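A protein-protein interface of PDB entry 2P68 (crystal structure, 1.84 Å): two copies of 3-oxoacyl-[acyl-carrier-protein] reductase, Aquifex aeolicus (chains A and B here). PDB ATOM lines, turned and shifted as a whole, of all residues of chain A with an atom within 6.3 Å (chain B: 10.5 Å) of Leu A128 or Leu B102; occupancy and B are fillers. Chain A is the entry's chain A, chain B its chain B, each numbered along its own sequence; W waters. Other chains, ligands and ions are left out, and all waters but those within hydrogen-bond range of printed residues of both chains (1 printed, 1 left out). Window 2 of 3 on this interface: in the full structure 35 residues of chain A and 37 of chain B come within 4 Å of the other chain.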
ATOM      1  N   TYR A  80     -20.506 -14.975 -18.294  1.00  0.00           N
ATOM      2  CA  TYR A  80     -21.463 -15.084 -19.389  1.00  0.00           C
ATOM      3  C   TYR A  80     -22.231 -16.415 -19.402  1.00  0.00           C
ATOM      4  O   TYR A  80     -23.211 -16.565 -20.131  1.00  0.00           O
ATOM      5  CB  TYR A  80     -20.786 -14.804 -20.735  1.00  0.00           C
ATOM      6  CG  TYR A  80     -20.558 -13.321 -21.005  1.00  0.00           C
ATOM      7  CD1 TYR A  80     -21.637 -12.456 -21.242  1.00  0.00           C
ATOM      8  CD2 TYR A  80     -19.272 -12.784 -21.028  1.00  0.00           C
ATOM      9  CE1 TYR A  80     -21.428 -11.084 -21.490  1.00  0.00           C
ATOM     10  CE2 TYR A  80     -19.054 -11.422 -21.280  1.00  0.00           C
ATOM     11  CZ  TYR A  80     -20.130 -10.581 -21.508  1.00  0.00           C
ATOM     12  OH  TYR A  80     -19.920  -9.237 -21.755  1.00  0.00           O
ATOM     13  N   ILE A  86     -23.777  -7.917 -19.231  1.00  0.00           N
ATOM     14  CA  ILE A  86     -23.499  -6.892 -18.229  1.00  0.00           C
ATOM     15  C   ILE A  86     -24.078  -5.542 -18.692  1.00  0.00           C
ATOM     16  O   ILE A  86     -23.837  -5.112 -19.816  1.00  0.00           O
ATOM     17  CB  ILE A  86     -21.984  -6.792 -17.970  1.00  0.00           C
ATOM     18  CG1 ILE A  86     -21.476  -8.091 -17.307  1.00  0.00           C
ATOM     19  CG2 ILE A  86     -21.644  -5.557 -17.105  1.00  0.00           C
ATOM     20  CD1 ILE A  86     -19.989  -8.258 -17.363  1.00  0.00           C
ATOM     21  N   VAL A 123     -11.194  -5.497 -18.918  1.00  0.00           N
ATOM     22  CA  VAL A 123     -12.511  -5.713 -18.285  1.00  0.00           C
ATOM     23  C   VAL A 123     -13.607  -4.953 -19.081  1.00  0.00           C
ATOM     24  O   VAL A 123     -14.707  -5.465 -19.318  1.00  0.00           O
ATOM     25  CB  VAL A 123     -12.483  -5.296 -16.784  1.00  0.00           C
ATOM     26  CG1 VAL A 123     -13.872  -5.361 -16.168  1.00  0.00           C
ATOM     27  CG2 VAL A 123     -11.517  -6.198 -15.992  1.00  0.00           C
ATOM     28  N   THR A 124     -13.288  -3.740 -19.514  1.00  0.00           N
ATOM     29  CA  THR A 124     -14.258  -2.917 -20.239  1.00  0.00           C
ATOM     30  C   THR A 124     -14.587  -3.560 -21.595  1.00  0.00           C
ATOM     31  O   THR A 124     -15.762  -3.734 -21.945  1.00  0.00           O
ATOM     32  CB  THR A 124     -13.766  -1.460 -20.421  1.00  0.00           C
ATOM     33  OG1 THR A 124     -13.539  -0.871 -19.128  1.00  0.00           O
ATOM     34  CG2 THR A 124     -14.816  -0.626 -21.185  1.00  0.00           C
ATOM     35  N   GLN A 125     -13.553  -3.938 -22.334  1.00  0.00           N
ATOM     36  CA  GLN A 125     -13.749  -4.632 -23.611  1.00  0.00           C
ATOM     37  C   GLN A 125     -14.649  -5.866 -23.454  1.00  0.00           C
ATOM     38  O   GLN A 125     -15.571  -6.069 -24.240  1.00  0.00           O
ATOM     39  CB  GLN A 125     -12.409  -5.027 -24.231  1.00  0.00           C
ATOM     40  CG  GLN A 125     -12.517  -5.452 -25.692  1.00  0.00           C
ATOM     41  CD  GLN A 125     -12.686  -4.273 -26.627  1.00  0.00           C
ATOM     42  OE1 GLN A 125     -13.806  -3.801 -26.864  1.00  0.00           O
ATOM     43  NE2 GLN A 125     -11.566  -3.782 -27.165  1.00  0.00           N
ATOM     44  N   ASN A 126     -14.389  -6.652 -22.422  1.00  0.00           N
ATOM     45  CA  ASN A 126     -15.159  -7.864 -22.105  1.00  0.00           C
ATOM     46  C   ASN A 126     -16.626  -7.626 -21.722  1.00  0.00           C
ATOM     47  O   ASN A 126     -17.464  -8.534 -21.850  1.00  0.00           O
ATOM     48  CB  ASN A 126     -14.465  -8.615 -20.963  1.00  0.00           C
ATOM     49  CG  ASN A 126     -13.381  -9.569 -21.446  1.00  0.00           C
ATOM     50  OD1 ASN A 126     -13.791 -10.671 -22.074  1.00  0.00           O
ATOM     51  ND2 ASN A 126     -12.186  -9.314 -21.259  1.00  0.00           N
ATOM     52  N   SER A 127     -16.933  -6.417 -21.243  1.00  0.00           N
ATOM     53  CA  SER A 127     -18.240  -6.111 -20.645  1.00  0.00           C
ATOM     54  C   SER A 127     -19.227  -5.408 -21.587  1.00  0.00           C
ATOM     55  O   SER A 127     -20.405  -5.323 -21.275  1.00  0.00           O
ATOM     56  CB  SER A 127     -18.059  -5.240 -19.386  1.00  0.00           C
ATOM     57  OG  SER A 127     -17.268  -5.893 -18.394  1.00  0.00           O
ATOM     58  N   LEU A 128     -18.746  -4.899 -22.721  1.00  0.00           N
ATOM     59  CA  LEU A 128     -19.568  -4.047 -23.590  1.00  0.00           C
ATOM     60  C   LEU A 128     -20.698  -4.705 -24.384  1.00  0.00           C
ATOM     61  O   LEU A 128     -21.646  -4.020 -24.785  1.00  0.00           O
ATOM     62  CB  LEU A 128     -18.674  -3.273 -24.564  1.00  0.00           C
ATOM     63  CG  LEU A 128     -17.860  -2.142 -23.940  1.00  0.00           C
ATOM     64  CD1 LEU A 128     -16.845  -1.615 -24.952  1.00  0.00           C
ATOM     65  CD2 LEU A 128     -18.777  -1.029 -23.440  1.00  0.00           C
ATOM     66  N   ARG A 129     -20.588  -6.009 -24.639  1.00  0.00           N
ATOM     67  CA  ARG A 129     -21.481  -6.670 -25.595  1.00  0.00           C
ATOM     68  C   ARG A 129     -22.951  -6.316 -25.409  1.00  0.00           C
ATOM     69  O   ARG A 129     -23.581  -5.803 -26.328  1.00  0.00           O
ATOM     70  CB  ARG A 129     -21.289  -8.193 -25.586  1.00  0.00           C
ATOM     71  CG  ARG A 129     -22.226  -8.915 -26.561  1.00  0.00           C
ATOM     72  CD  ARG A 129     -21.791 -10.344 -26.757  1.00  0.00           C
ATOM     73  NE  ARG A 129     -22.611 -11.019 -27.760  1.00  0.00           N
ATOM     74  CZ  ARG A 129     -22.745 -12.337 -27.853  1.00  0.00           C
ATOM     75  NH1 ARG A 129     -22.114 -13.137 -27.003  1.00  0.00           N
ATOM     76  NH2 ARG A 129     -23.521 -12.855 -28.796  1.00  0.00           N
ATOM     77  N   LYS A 130     -23.496  -6.589 -24.227  1.00  0.00           N
ATOM     78  CA  LYS A 130     -24.937  -6.373 -24.011  1.00  0.00           C
ATOM     79  C   LYS A 130     -25.306  -4.884 -24.055  1.00  0.00           C
ATOM     80  O   LYS A 130     -26.384  -4.515 -24.538  1.00  0.00           O
ATOM     81  CB  LYS A 130     -25.389  -7.007 -22.698  1.00  0.00           C
ATOM     82  CG  LYS A 130     -26.895  -6.999 -22.510  1.00  0.00           C
ATOM     83  CD  LYS A 130     -27.293  -7.836 -21.312  1.00  0.00           C
ATOM     84  CE  LYS A 130     -28.807  -7.918 -21.200  1.00  0.00           C
ATOM     85  NZ  LYS A 130     -29.362  -6.718 -20.523  1.00  0.00           N
ATOM     86  N   MET A 131     -24.396  -4.037 -23.567  1.00  0.00           N
ATOM     87  CA  MET A 131     -24.604  -2.588 -23.543  1.00  0.00           C
ATOM     88  C   MET A 131     -24.764  -2.016 -24.953  1.00  0.00           C
ATOM     89  O   MET A 131     -25.680  -1.222 -25.215  1.00  0.00           O
ATOM     90  CB  MET A 131     -23.432  -1.866 -22.856  1.00  0.00           C
ATOM     91  CG  MET A 131     -23.155  -2.277 -21.403  1.00  0.00           C
ATOM     92  SD  MET A 131     -21.744  -1.343 -20.755  1.00  0.00           S
ATOM     93  CE  MET A 131     -21.301  -2.299 -19.301  1.00  0.00           C
ATOM     94  N   ILE A 132     -23.850  -2.392 -25.849  1.00  0.00           N
ATOM     95  CA  ILE A 132     -23.890  -1.919 -27.233  1.00  0.00           C
ATOM     96  C   ILE A 132     -25.149  -2.439 -27.943  1.00  0.00           C
ATOM     97  O   ILE A 132     -25.841  -1.682 -28.633  1.00  0.00           O
ATOM     98  CB  ILE A 132     -22.600  -2.323 -28.008  1.00  0.00           C
ATOM     99  CG1 ILE A 132     -21.358  -1.723 -27.329  1.00  0.00           C
ATOM    100  CG2 ILE A 132     -22.658  -1.860 -29.468  1.00  0.00           C
ATOM    101  CD1 ILE A 132     -21.355  -0.214 -27.271  1.00  0.00           C
ATOM    102  N   LYS A 133     -25.443  -3.720 -27.747  1.00  0.00           N
ATOM    103  CA  LYS A 133     -26.616  -4.366 -28.355  1.00  0.00           C
ATOM    104  C   LYS A 133     -27.912  -3.639 -28.010  1.00  0.00           C
ATOM    105  O   LYS A 133     -28.720  -3.341 -28.891  1.00  0.00           O
ATOM    106  CB  LYS A 133     -26.717  -5.825 -27.886  1.00  0.00           C
ATOM    107  CG  LYS A 133     -27.806  -6.635 -28.594  1.00  0.00           C
ATOM    108  CD  LYS A 133     -27.998  -7.991 -27.924  1.00  0.00           C
ATOM    109  CE  LYS A 133     -28.912  -8.919 -28.731  1.00  0.00           C
ATOM    110  NZ  LYS A 133     -30.237  -8.299 -29.050  1.00  0.00           N
ATOM    111  N   ILE A 139     -20.620   2.713 -17.668  1.00  0.00           N
ATOM    112  CA  ILE A 139     -19.294   2.306 -17.227  1.00  0.00           C
ATOM    113  C   ILE A 139     -18.786   3.397 -16.287  1.00  0.00           C
ATOM    114  O   ILE A 139     -18.802   4.586 -16.632  1.00  0.00           O
ATOM    115  CB  ILE A 139     -18.333   2.133 -18.423  1.00  0.00           C
ATOM    116  CG1 ILE A 139     -18.792   0.960 -19.290  1.00  0.00           C
ATOM    117  CG2 ILE A 139     -16.872   1.944 -17.941  1.00  0.00           C
ATOM    118  CD1 ILE A 139     -18.312   1.071 -20.721  1.00  0.00           C
ATOM    119  N   LEU A 171     -13.413   7.036 -24.501  1.00  0.00           N
ATOM    120  CA  LEU A 171     -14.406   5.978 -24.624  1.00  0.00           C
ATOM    121  C   LEU A 171     -15.815   6.548 -24.630  1.00  0.00           C
ATOM    122  O   LEU A 171     -16.686   6.049 -25.336  1.00  0.00           O
ATOM    123  CB  LEU A 171     -14.245   4.949 -23.513  1.00  0.00           C
ATOM    124  CG  LEU A 171     -15.064   3.663 -23.695  1.00  0.00           C
ATOM    125  CD1 LEU A 171     -14.760   2.968 -25.032  1.00  0.00           C
ATOM    126  CD2 LEU A 171     -14.787   2.744 -22.516  1.00  0.00           C
ATOM    127  N   GLU A 174     -16.637   7.669 -28.130  1.00  0.00           N
ATOM    128  CA  GLU A 174     -16.826   6.525 -29.037  1.00  0.00           C
ATOM    129  C   GLU A 174     -18.158   5.799 -28.846  1.00  0.00           C
ATOM    130  O   GLU A 174     -18.789   5.354 -29.822  1.00  0.00           O
ATOM    131  CB  GLU A 174     -15.690   5.534 -28.856  1.00  0.00           C
ATOM    132  CG  GLU A 174     -14.403   6.003 -29.475  1.00  0.00           C
ATOM    133  CD  GLU A 174     -13.429   4.871 -29.679  1.00  0.00           C
ATOM    134  OE1 GLU A 174     -13.840   3.694 -29.617  1.00  0.00           O
ATOM    135  OE2 GLU A 174     -12.253   5.164 -29.919  1.00  0.00           O
ATOM    136  N   LEU A 175     -18.597   5.707 -27.595  1.00  0.00           N
ATOM    137  CA  LEU A 175     -19.801   4.943 -27.260  1.00  0.00           C
ATOM    138  C   LEU A 175     -21.077   5.756 -27.145  1.00  0.00           C
ATOM    139  O   LEU A 175     -22.177   5.191 -27.051  1.00  0.00           O
ATOM    140  CB  LEU A 175     -19.577   4.156 -25.971  1.00  0.00           C
ATOM    141  CG  LEU A 175     -18.414   3.160 -25.939  1.00  0.00           C
ATOM    142  CD1 LEU A 175     -18.412   2.408 -24.617  1.00  0.00           C
ATOM    143  CD2 LEU A 175     -18.481   2.175 -27.092  1.00  0.00           C
ATOM    144  N   VAL A 180     -24.188   4.404 -24.448  1.00  0.00           N
ATOM    145  CA  VAL A 180     -23.424   3.786 -23.363  1.00  0.00           C
ATOM    146  C   VAL A 180     -22.599   4.897 -22.730  1.00  0.00           C
ATOM    147  O   VAL A 180     -21.699   5.461 -23.369  1.00  0.00           O
ATOM    148  CB  VAL A 180     -22.542   2.635 -23.879  1.00  0.00           C
ATOM    149  CG1 VAL A 180     -21.688   2.032 -22.745  1.00  0.00           C
ATOM    150  CG2 VAL A 180     -23.428   1.564 -24.511  1.00  0.00           C
ATOM    151  N   ARG B  97      -1.384   3.990 -32.025  1.00  0.00           N
ATOM    152  CA  ARG B  97      -1.884   2.815 -32.712  1.00  0.00           C
ATOM    153  C   ARG B  97      -3.394   2.981 -32.718  1.00  0.00           C
ATOM    154  O   ARG B  97      -4.110   2.422 -31.876  1.00  0.00           O
ATOM    155  CB  ARG B  97      -1.450   1.520 -32.017  1.00  0.00           C
ATOM    156  CG  ARG B  97       0.073   1.279 -31.979  1.00  0.00           C
ATOM    157  CD  ARG B  97       0.655   0.898 -33.343  1.00  0.00           C
ATOM    158  NE  ARG B  97       2.097   0.674 -33.247  1.00  0.00           N
ATOM    159  CZ  ARG B  97       3.036   1.567 -33.553  1.00  0.00           C
ATOM    160  NH1 ARG B  97       2.710   2.773 -34.004  1.00  0.00           N
ATOM    161  NH2 ARG B  97       4.316   1.245 -33.415  1.00  0.00           N
ATOM    162  N   ASP B  98      -3.859   3.796 -33.663  1.00  0.00           N
ATOM    163  CA  ASP B  98      -5.241   4.256 -33.691  1.00  0.00           C
ATOM    164  C   ASP B  98      -6.192   3.141 -34.085  1.00  0.00           C
ATOM    165  O   ASP B  98      -6.034   2.534 -35.137  1.00  0.00           O
ATOM    166  CB  ASP B  98      -5.408   5.423 -34.669  1.00  0.00           C
ATOM    167  CG  ASP B  98      -4.672   6.677 -34.232  1.00  0.00           C
ATOM    168  OD1 ASP B  98      -4.207   6.757 -33.072  1.00  0.00           O
ATOM    169  OD2 ASP B  98      -4.578   7.599 -35.062  1.00  0.00           O
ATOM    170  N   LYS B  99      -7.167   2.867 -33.227  1.00  0.00           N
ATOM    171  CA  LYS B  99      -8.213   1.889 -33.526  1.00  0.00           C
ATOM    172  C   LYS B  99      -9.446   2.281 -32.720  1.00  0.00           C
ATOM    173  O   LYS B  99      -9.321   2.729 -31.580  1.00  0.00           O
ATOM    174  CB  LYS B  99      -7.792   0.468 -33.114  1.00  0.00           C
ATOM    175  CG  LYS B  99      -6.534  -0.135 -33.767  1.00  0.00           C
ATOM    176  CD  LYS B  99      -6.765  -0.625 -35.212  1.00  0.00           C
ATOM    177  CE  LYS B  99      -7.585  -1.908 -35.279  1.00  0.00           C
ATOM    178  NZ  LYS B  99      -8.015  -2.228 -36.681  1.00  0.00           N
ATOM    179  N   LEU B 100     -10.637   2.108 -33.299  1.00  0.00           N
ATOM    180  CA  LEU B 100     -11.859   2.166 -32.500  1.00  0.00           C
ATOM    181  C   LEU B 100     -11.728   1.161 -31.348  1.00  0.00           C
ATOM    182  O   LEU B 100     -11.206   0.061 -31.524  1.00  0.00           O
ATOM    183  CB  LEU B 100     -13.104   1.866 -33.350  1.00  0.00           C
ATOM    184  CG  LEU B 100     -13.561   2.926 -34.360  1.00  0.00           C
ATOM    185  CD1 LEU B 100     -14.841   2.482 -35.072  1.00  0.00           C
ATOM    186  CD2 LEU B 100     -13.768   4.276 -33.692  1.00  0.00           C
ATOM    187  N   PHE B 101     -12.184   1.545 -30.162  1.00  0.00           N
ATOM    188  CA  PHE B 101     -12.020   0.705 -28.976  1.00  0.00           C
ATOM    189  C   PHE B 101     -12.434  -0.751 -29.201  1.00  0.00           C
ATOM    190  O   PHE B 101     -11.715  -1.684 -28.828  1.00  0.00           O
ATOM    191  CB  PHE B 101     -12.800   1.294 -27.798  1.00  0.00           C
ATOM    192  CG  PHE B 101     -12.545   0.598 -26.499  1.00  0.00           C
ATOM    193  CD1 PHE B 101     -11.421   0.918 -25.746  1.00  0.00           C
ATOM    194  CD2 PHE B 101     -13.439  -0.349 -26.005  1.00  0.00           C
ATOM    195  CE1 PHE B 101     -11.178   0.300 -24.542  1.00  0.00           C
ATOM    196  CE2 PHE B 101     -13.198  -0.981 -24.786  1.00  0.00           C
ATOM    197  CZ  PHE B 101     -12.067  -0.657 -24.056  1.00  0.00           C
ATOM    198  N   LEU B 102     -13.593  -0.929 -29.827  1.00  0.00           N
ATOM    199  CA  LEU B 102     -14.152  -2.254 -30.065  1.00  0.00           C
ATOM    200  C   LEU B 102     -13.331  -3.059 -31.083  1.00  0.00           C
ATOM    201  O   LEU B 102     -13.552  -4.260 -31.247  1.00  0.00           O
ATOM    202  CB  LEU B 102     -15.613  -2.133 -30.523  1.00  0.00           C
ATOM    203  CG  LEU B 102     -16.659  -1.749 -29.468  1.00  0.00           C
ATOM    204  CD1 LEU B 102     -17.932  -1.242 -30.139  1.00  0.00           C
ATOM    205  CD2 LEU B 102     -16.955  -2.941 -28.540  1.00  0.00           C
ATOM    206  N   ARG B 103     -12.394  -2.395 -31.761  1.00  0.00           N
ATOM    207  CA  ARG B 103     -11.467  -3.060 -32.681  1.00  0.00           C
ATOM    208  C   ARG B 103     -10.017  -3.051 -32.172  1.00  0.00           C
ATOM    209  O   ARG B 103      -9.097  -3.423 -32.899  1.00  0.00           O
ATOM    210  CB  ARG B 103     -11.512  -2.397 -34.063  1.00  0.00           C
ATOM    211  CG  ARG B 103     -12.907  -2.161 -34.637  1.00  0.00           C
ATOM    212  CD  ARG B 103     -13.694  -3.449 -34.830  1.00  0.00           C
ATOM    213  NE  ARG B 103     -12.935  -4.453 -35.567  1.00  0.00           N
ATOM    214  CZ  ARG B 103     -12.708  -5.686 -35.138  1.00  0.00           C
ATOM    215  NH1 ARG B 103     -13.200  -6.092 -33.967  1.00  0.00           N
ATOM    216  NH2 ARG B 103     -12.002  -6.518 -35.893  1.00  0.00           N
ATOM    217  N   MET B 104      -9.809  -2.632 -30.928  1.00  0.00           N
ATOM    218  CA  MET B 104      -8.453  -2.483 -30.403  1.00  0.00           C
ATOM    219  C   MET B 104      -7.912  -3.785 -29.820  1.00  0.00           C
ATOM    220  O   MET B 104      -8.558  -4.397 -28.970  1.00  0.00           O
ATOM    221  CB  MET B 104      -8.424  -1.378 -29.341  1.00  0.00           C
ATOM    222  CG  MET B 104      -7.022  -1.011 -28.865  1.00  0.00           C
ATOM    223  SD  MET B 104      -7.019   0.466 -27.817  1.00  0.00           S
ATOM    224  CE  MET B 104      -7.415   1.728 -29.041  1.00  0.00           C
ATOM    225  N   SER B 105      -6.729  -4.205 -30.274  1.00  0.00           N
ATOM    226  CA  SER B 105      -6.077  -5.397 -29.722  1.00  0.00           C
ATOM    227  C   SER B 105      -5.312  -5.063 -28.446  1.00  0.00           C
ATOM    228  O   SER B 105      -4.959  -3.897 -28.212  1.00  0.00           O
ATOM    229  CB  SER B 105      -5.123  -6.032 -30.737  1.00  0.00           C
ATOM    230  OG  SER B 105      -3.892  -5.331 -30.791  1.00  0.00           O
ATOM    231  N   LEU B 106      -5.043  -6.089 -27.633  1.00  0.00           N
ATOM    232  CA  LEU B 106      -4.212  -5.916 -26.454  1.00  0.00           C
ATOM    233  C   LEU B 106      -2.861  -5.325 -26.847  1.00  0.00           C
ATOM    234  O   LEU B 106      -2.327  -4.485 -26.131  1.00  0.00           O
ATOM    235  CB  LEU B 106      -4.031  -7.237 -25.681  1.00  0.00           C
ATOM    236  CG  LEU B 106      -3.354  -7.133 -24.309  1.00  0.00           C
ATOM    237  CD1 LEU B 106      -4.046  -6.096 -23.401  1.00  0.00           C
ATOM    238  CD2 LEU B 106      -3.330  -8.496 -23.636  1.00  0.00           C
ATOM    239  N   ASP B 108      -2.262  -3.366 -29.560  1.00  0.00           N
ATOM    240  CA  ASP B 108      -2.561  -1.971 -29.921  1.00  0.00           C
ATOM    241  C   ASP B 108      -2.505  -1.112 -28.651  1.00  0.00           C
ATOM    242  O   ASP B 108      -1.968  -0.002 -28.654  1.00  0.00           O
ATOM    243  CB  ASP B 108      -3.964  -1.819 -30.522  1.00  0.00           C
ATOM    244  CG  ASP B 108      -4.105  -2.412 -31.925  1.00  0.00           C
ATOM    245  OD1 ASP B 108      -3.125  -2.387 -32.703  1.00  0.00           O
ATOM    246  OD2 ASP B 108      -5.231  -2.873 -32.251  1.00  0.00           O
ATOM    247  N   TRP B 109      -3.074  -1.644 -27.572  1.00  0.00           N
ATOM    248  CA  TRP B 109      -3.094  -0.959 -26.274  1.00  0.00           C
ATOM    249  C   TRP B 109      -1.736  -0.974 -25.569  1.00  0.00           C
ATOM    250  O   TRP B 109      -1.196   0.081 -25.203  1.00  0.00           O
ATOM    251  CB  TRP B 109      -4.155  -1.606 -25.378  1.00  0.00           C
ATOM    252  CG  TRP B 109      -4.163  -1.103 -23.969  1.00  0.00           C
ATOM    253  CD1 TRP B 109      -3.490  -1.633 -22.904  1.00  0.00           C
ATOM    254  CD2 TRP B 109      -4.907   0.010 -23.463  1.00  0.00           C
ATOM    255  NE1 TRP B 109      -3.758  -0.905 -21.768  1.00  0.00           N
ATOM    256  CE2 TRP B 109      -4.624   0.108 -22.084  1.00  0.00           C
ATOM    257  CE3 TRP B 109      -5.782   0.940 -24.042  1.00  0.00           C
ATOM    258  CZ2 TRP B 109      -5.183   1.095 -21.277  1.00  0.00           C
ATOM    259  CZ3 TRP B 109      -6.333   1.931 -23.236  1.00  0.00           C
ATOM    260  CH2 TRP B 109      -6.045   1.990 -21.869  1.00  0.00           C
ATOM    261  N   VAL B 152     -11.915  10.075 -30.506  1.00  0.00           N
ATOM    262  CA  VAL B 152     -12.386   8.836 -31.114  1.00  0.00           C
ATOM    263  C   VAL B 152     -11.229   8.157 -31.851  1.00  0.00           C
ATOM    264  O   VAL B 152     -10.488   8.808 -32.590  1.00  0.00           O
ATOM    265  CB  VAL B 152     -13.576   9.103 -32.068  1.00  0.00           C
ATOM    266  CG1 VAL B 152     -13.964   7.837 -32.827  1.00  0.00           C
ATOM    267  CG2 VAL B 152     -14.769   9.642 -31.276  1.00  0.00           C
ATOM    268  N   GLY B 153     -11.061   6.863 -31.601  1.00  0.00           N
ATOM    269  CA  GLY B 153     -10.029   6.060 -32.245  1.00  0.00           C
ATOM    270  C   GLY B 153      -8.708   6.076 -31.492  1.00  0.00           C
ATOM    271  O   GLY B 153      -7.739   5.435 -31.913  1.00  0.00           O
ATOM    272  N   GLN B 154      -8.676   6.803 -30.376  1.00  0.00           N
ATOM    273  CA  GLN B 154      -7.444   7.022 -29.629  1.00  0.00           C
ATOM    274  C   GLN B 154      -7.576   6.786 -28.128  1.00  0.00           C
ATOM    275  O   GLN B 154      -6.923   7.442 -27.325  1.00  0.00           O
ATOM    276  CB  GLN B 154      -6.906   8.427 -29.915  1.00  0.00           C
ATOM    277  CG  GLN B 154      -6.438   8.604 -31.345  1.00  0.00           C
ATOM    278  CD  GLN B 154      -5.450   9.731 -31.497  1.00  0.00           C
ATOM    279  OE1 GLN B 154      -5.845  10.927 -31.069  1.00  0.00           O
ATOM    280  NE2 GLN B 154      -4.337   9.535 -31.999  1.00  0.00           N
ATOM    281  N   VAL B 155      -8.406   5.827 -27.735  1.00  0.00           N
ATOM    282  CA  VAL B 155      -8.548   5.555 -26.309  1.00  0.00           C
ATOM    283  C   VAL B 155      -7.179   5.214 -25.683  1.00  0.00           C
ATOM    284  O   VAL B 155      -6.884   5.630 -24.561  1.00  0.00           O
ATOM    285  CB  VAL B 155      -9.587   4.446 -26.034  1.00  0.00           C
ATOM    286  CG1 VAL B 155      -9.592   4.088 -24.567  1.00  0.00           C
ATOM    287  CG2 VAL B 155     -10.976   4.898 -26.469  1.00  0.00           C
ATOM    288  N   ASN B 156      -6.343   4.484 -26.422  1.00  0.00           N
ATOM    289  CA  ASN B 156      -5.010   4.119 -25.936  1.00  0.00           C
ATOM    290  C   ASN B 156      -4.074   5.320 -25.831  1.00  0.00           C
ATOM    291  O   ASN B 156      -3.449   5.548 -24.786  1.00  0.00           O
ATOM    292  CB  ASN B 156      -4.377   2.985 -26.782  1.00  0.00           C
ATOM    293  CG  ASN B 156      -4.427   3.244 -28.292  1.00  0.00           C
ATOM    294  OD1 ASN B 156      -5.033   4.207 -28.766  1.00  0.00           O
ATOM    295  ND2 ASN B 156      -3.796   2.354 -29.057  1.00  0.00           N
HETATM  296  O   HOH W   1     -15.473   1.644 -30.176  1.00  0.00           O
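Leu A128 touches just these residues of chain B: Phe B101 (3.7 Å) and Leu B102 (3.8 Å).
Leu B102 touches two residues of chain A.
Ser A127 touches none of the printed residues of chain B.
Printed residues of chain A within 4 Å of Met B104: Gln A125 (3.6 Å).
Of the printed residues of chain A, Leu B100 touches Glu A174 (3.7 Å).
The nearest residue of chain B that does not touch Leu A128 is Arg B103 (8.2 Å).
The nearest residue of chain A that does not touch Leu B102 is Ile A132 (4.5 Å).
The nearest printed residue of chain A that does not touch Phe B101 is Leu A175 (5.7 Å).
No position is printed for both chains.
Of the 14 pairs that touch across the chains among the printed residues, none has its exchanged pair printed and touching as well.
The side-chain carboxylate (OD1) of Asp B98 lies within hydrogen-bond range of the side-chain amide nitrogen (NE2) of Gln B154, 3.0 Å away.
N of Lys B99 sits at hydrogen-bond distance from O of Gly B153 (2.9 Å).
Hydrophobic or aromatic side chains of chain A within 4 Å of the printed part of chain B: Leu A128 and Leu A171.
Of the 17 printed residues of chain B, 8 touch a printed residue of chain A.
Among the printed residues, 14 pairs touch across the chains.
Among the printed residues, no Asp or Glu carboxylate lies within 4 Å of a Lys or Arg side-chain nitrogen of the other chain.
Water W1 lies within hydrogen-bond range of the side-chain carboxylate (OE1) of Glu A174, the backbone NH (N) of Leu B102 and the backbone NH (N) of Phe B101.
Among the printed residues, merely in contact across the chains: Leu A171 with Phe B101 (3.6 Å), Gln A125 with Met B104 (3.6 Å), Gln A125 with Leu B102 (3.6 Å), Glu A174 with Val B155 (3.7 Å), Leu A128 with Phe B101 (3.7 Å), Glu A174 with Val B152 (3.7 Å), Glu A174 with Leu B100 (3.7 Å), Leu A171 with Val B155 (3.8 Å), Leu A128 with Leu B102 (3.8 Å), Glu A174 with Gln B154 (3.96 Å) and Thr A124 with Phe B101 (3.96 Å).
The backbone carbonyl oxygen (O) of Phe B101 lies within hydrogen-bond range of the side-chain amide nitrogen (NE2) of Gln A125, 2.7 Å away.
The backbone NH of Phe B101 lies within hydrogen-bond range of the side-chain carboxylate of Glu A174, 2.8 Å away.
The side-chain carboxylate (OE2) of Glu A174 sits at hydrogen-bond distance from the backbone NH (N) of Gly B153 (2.7 Å).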
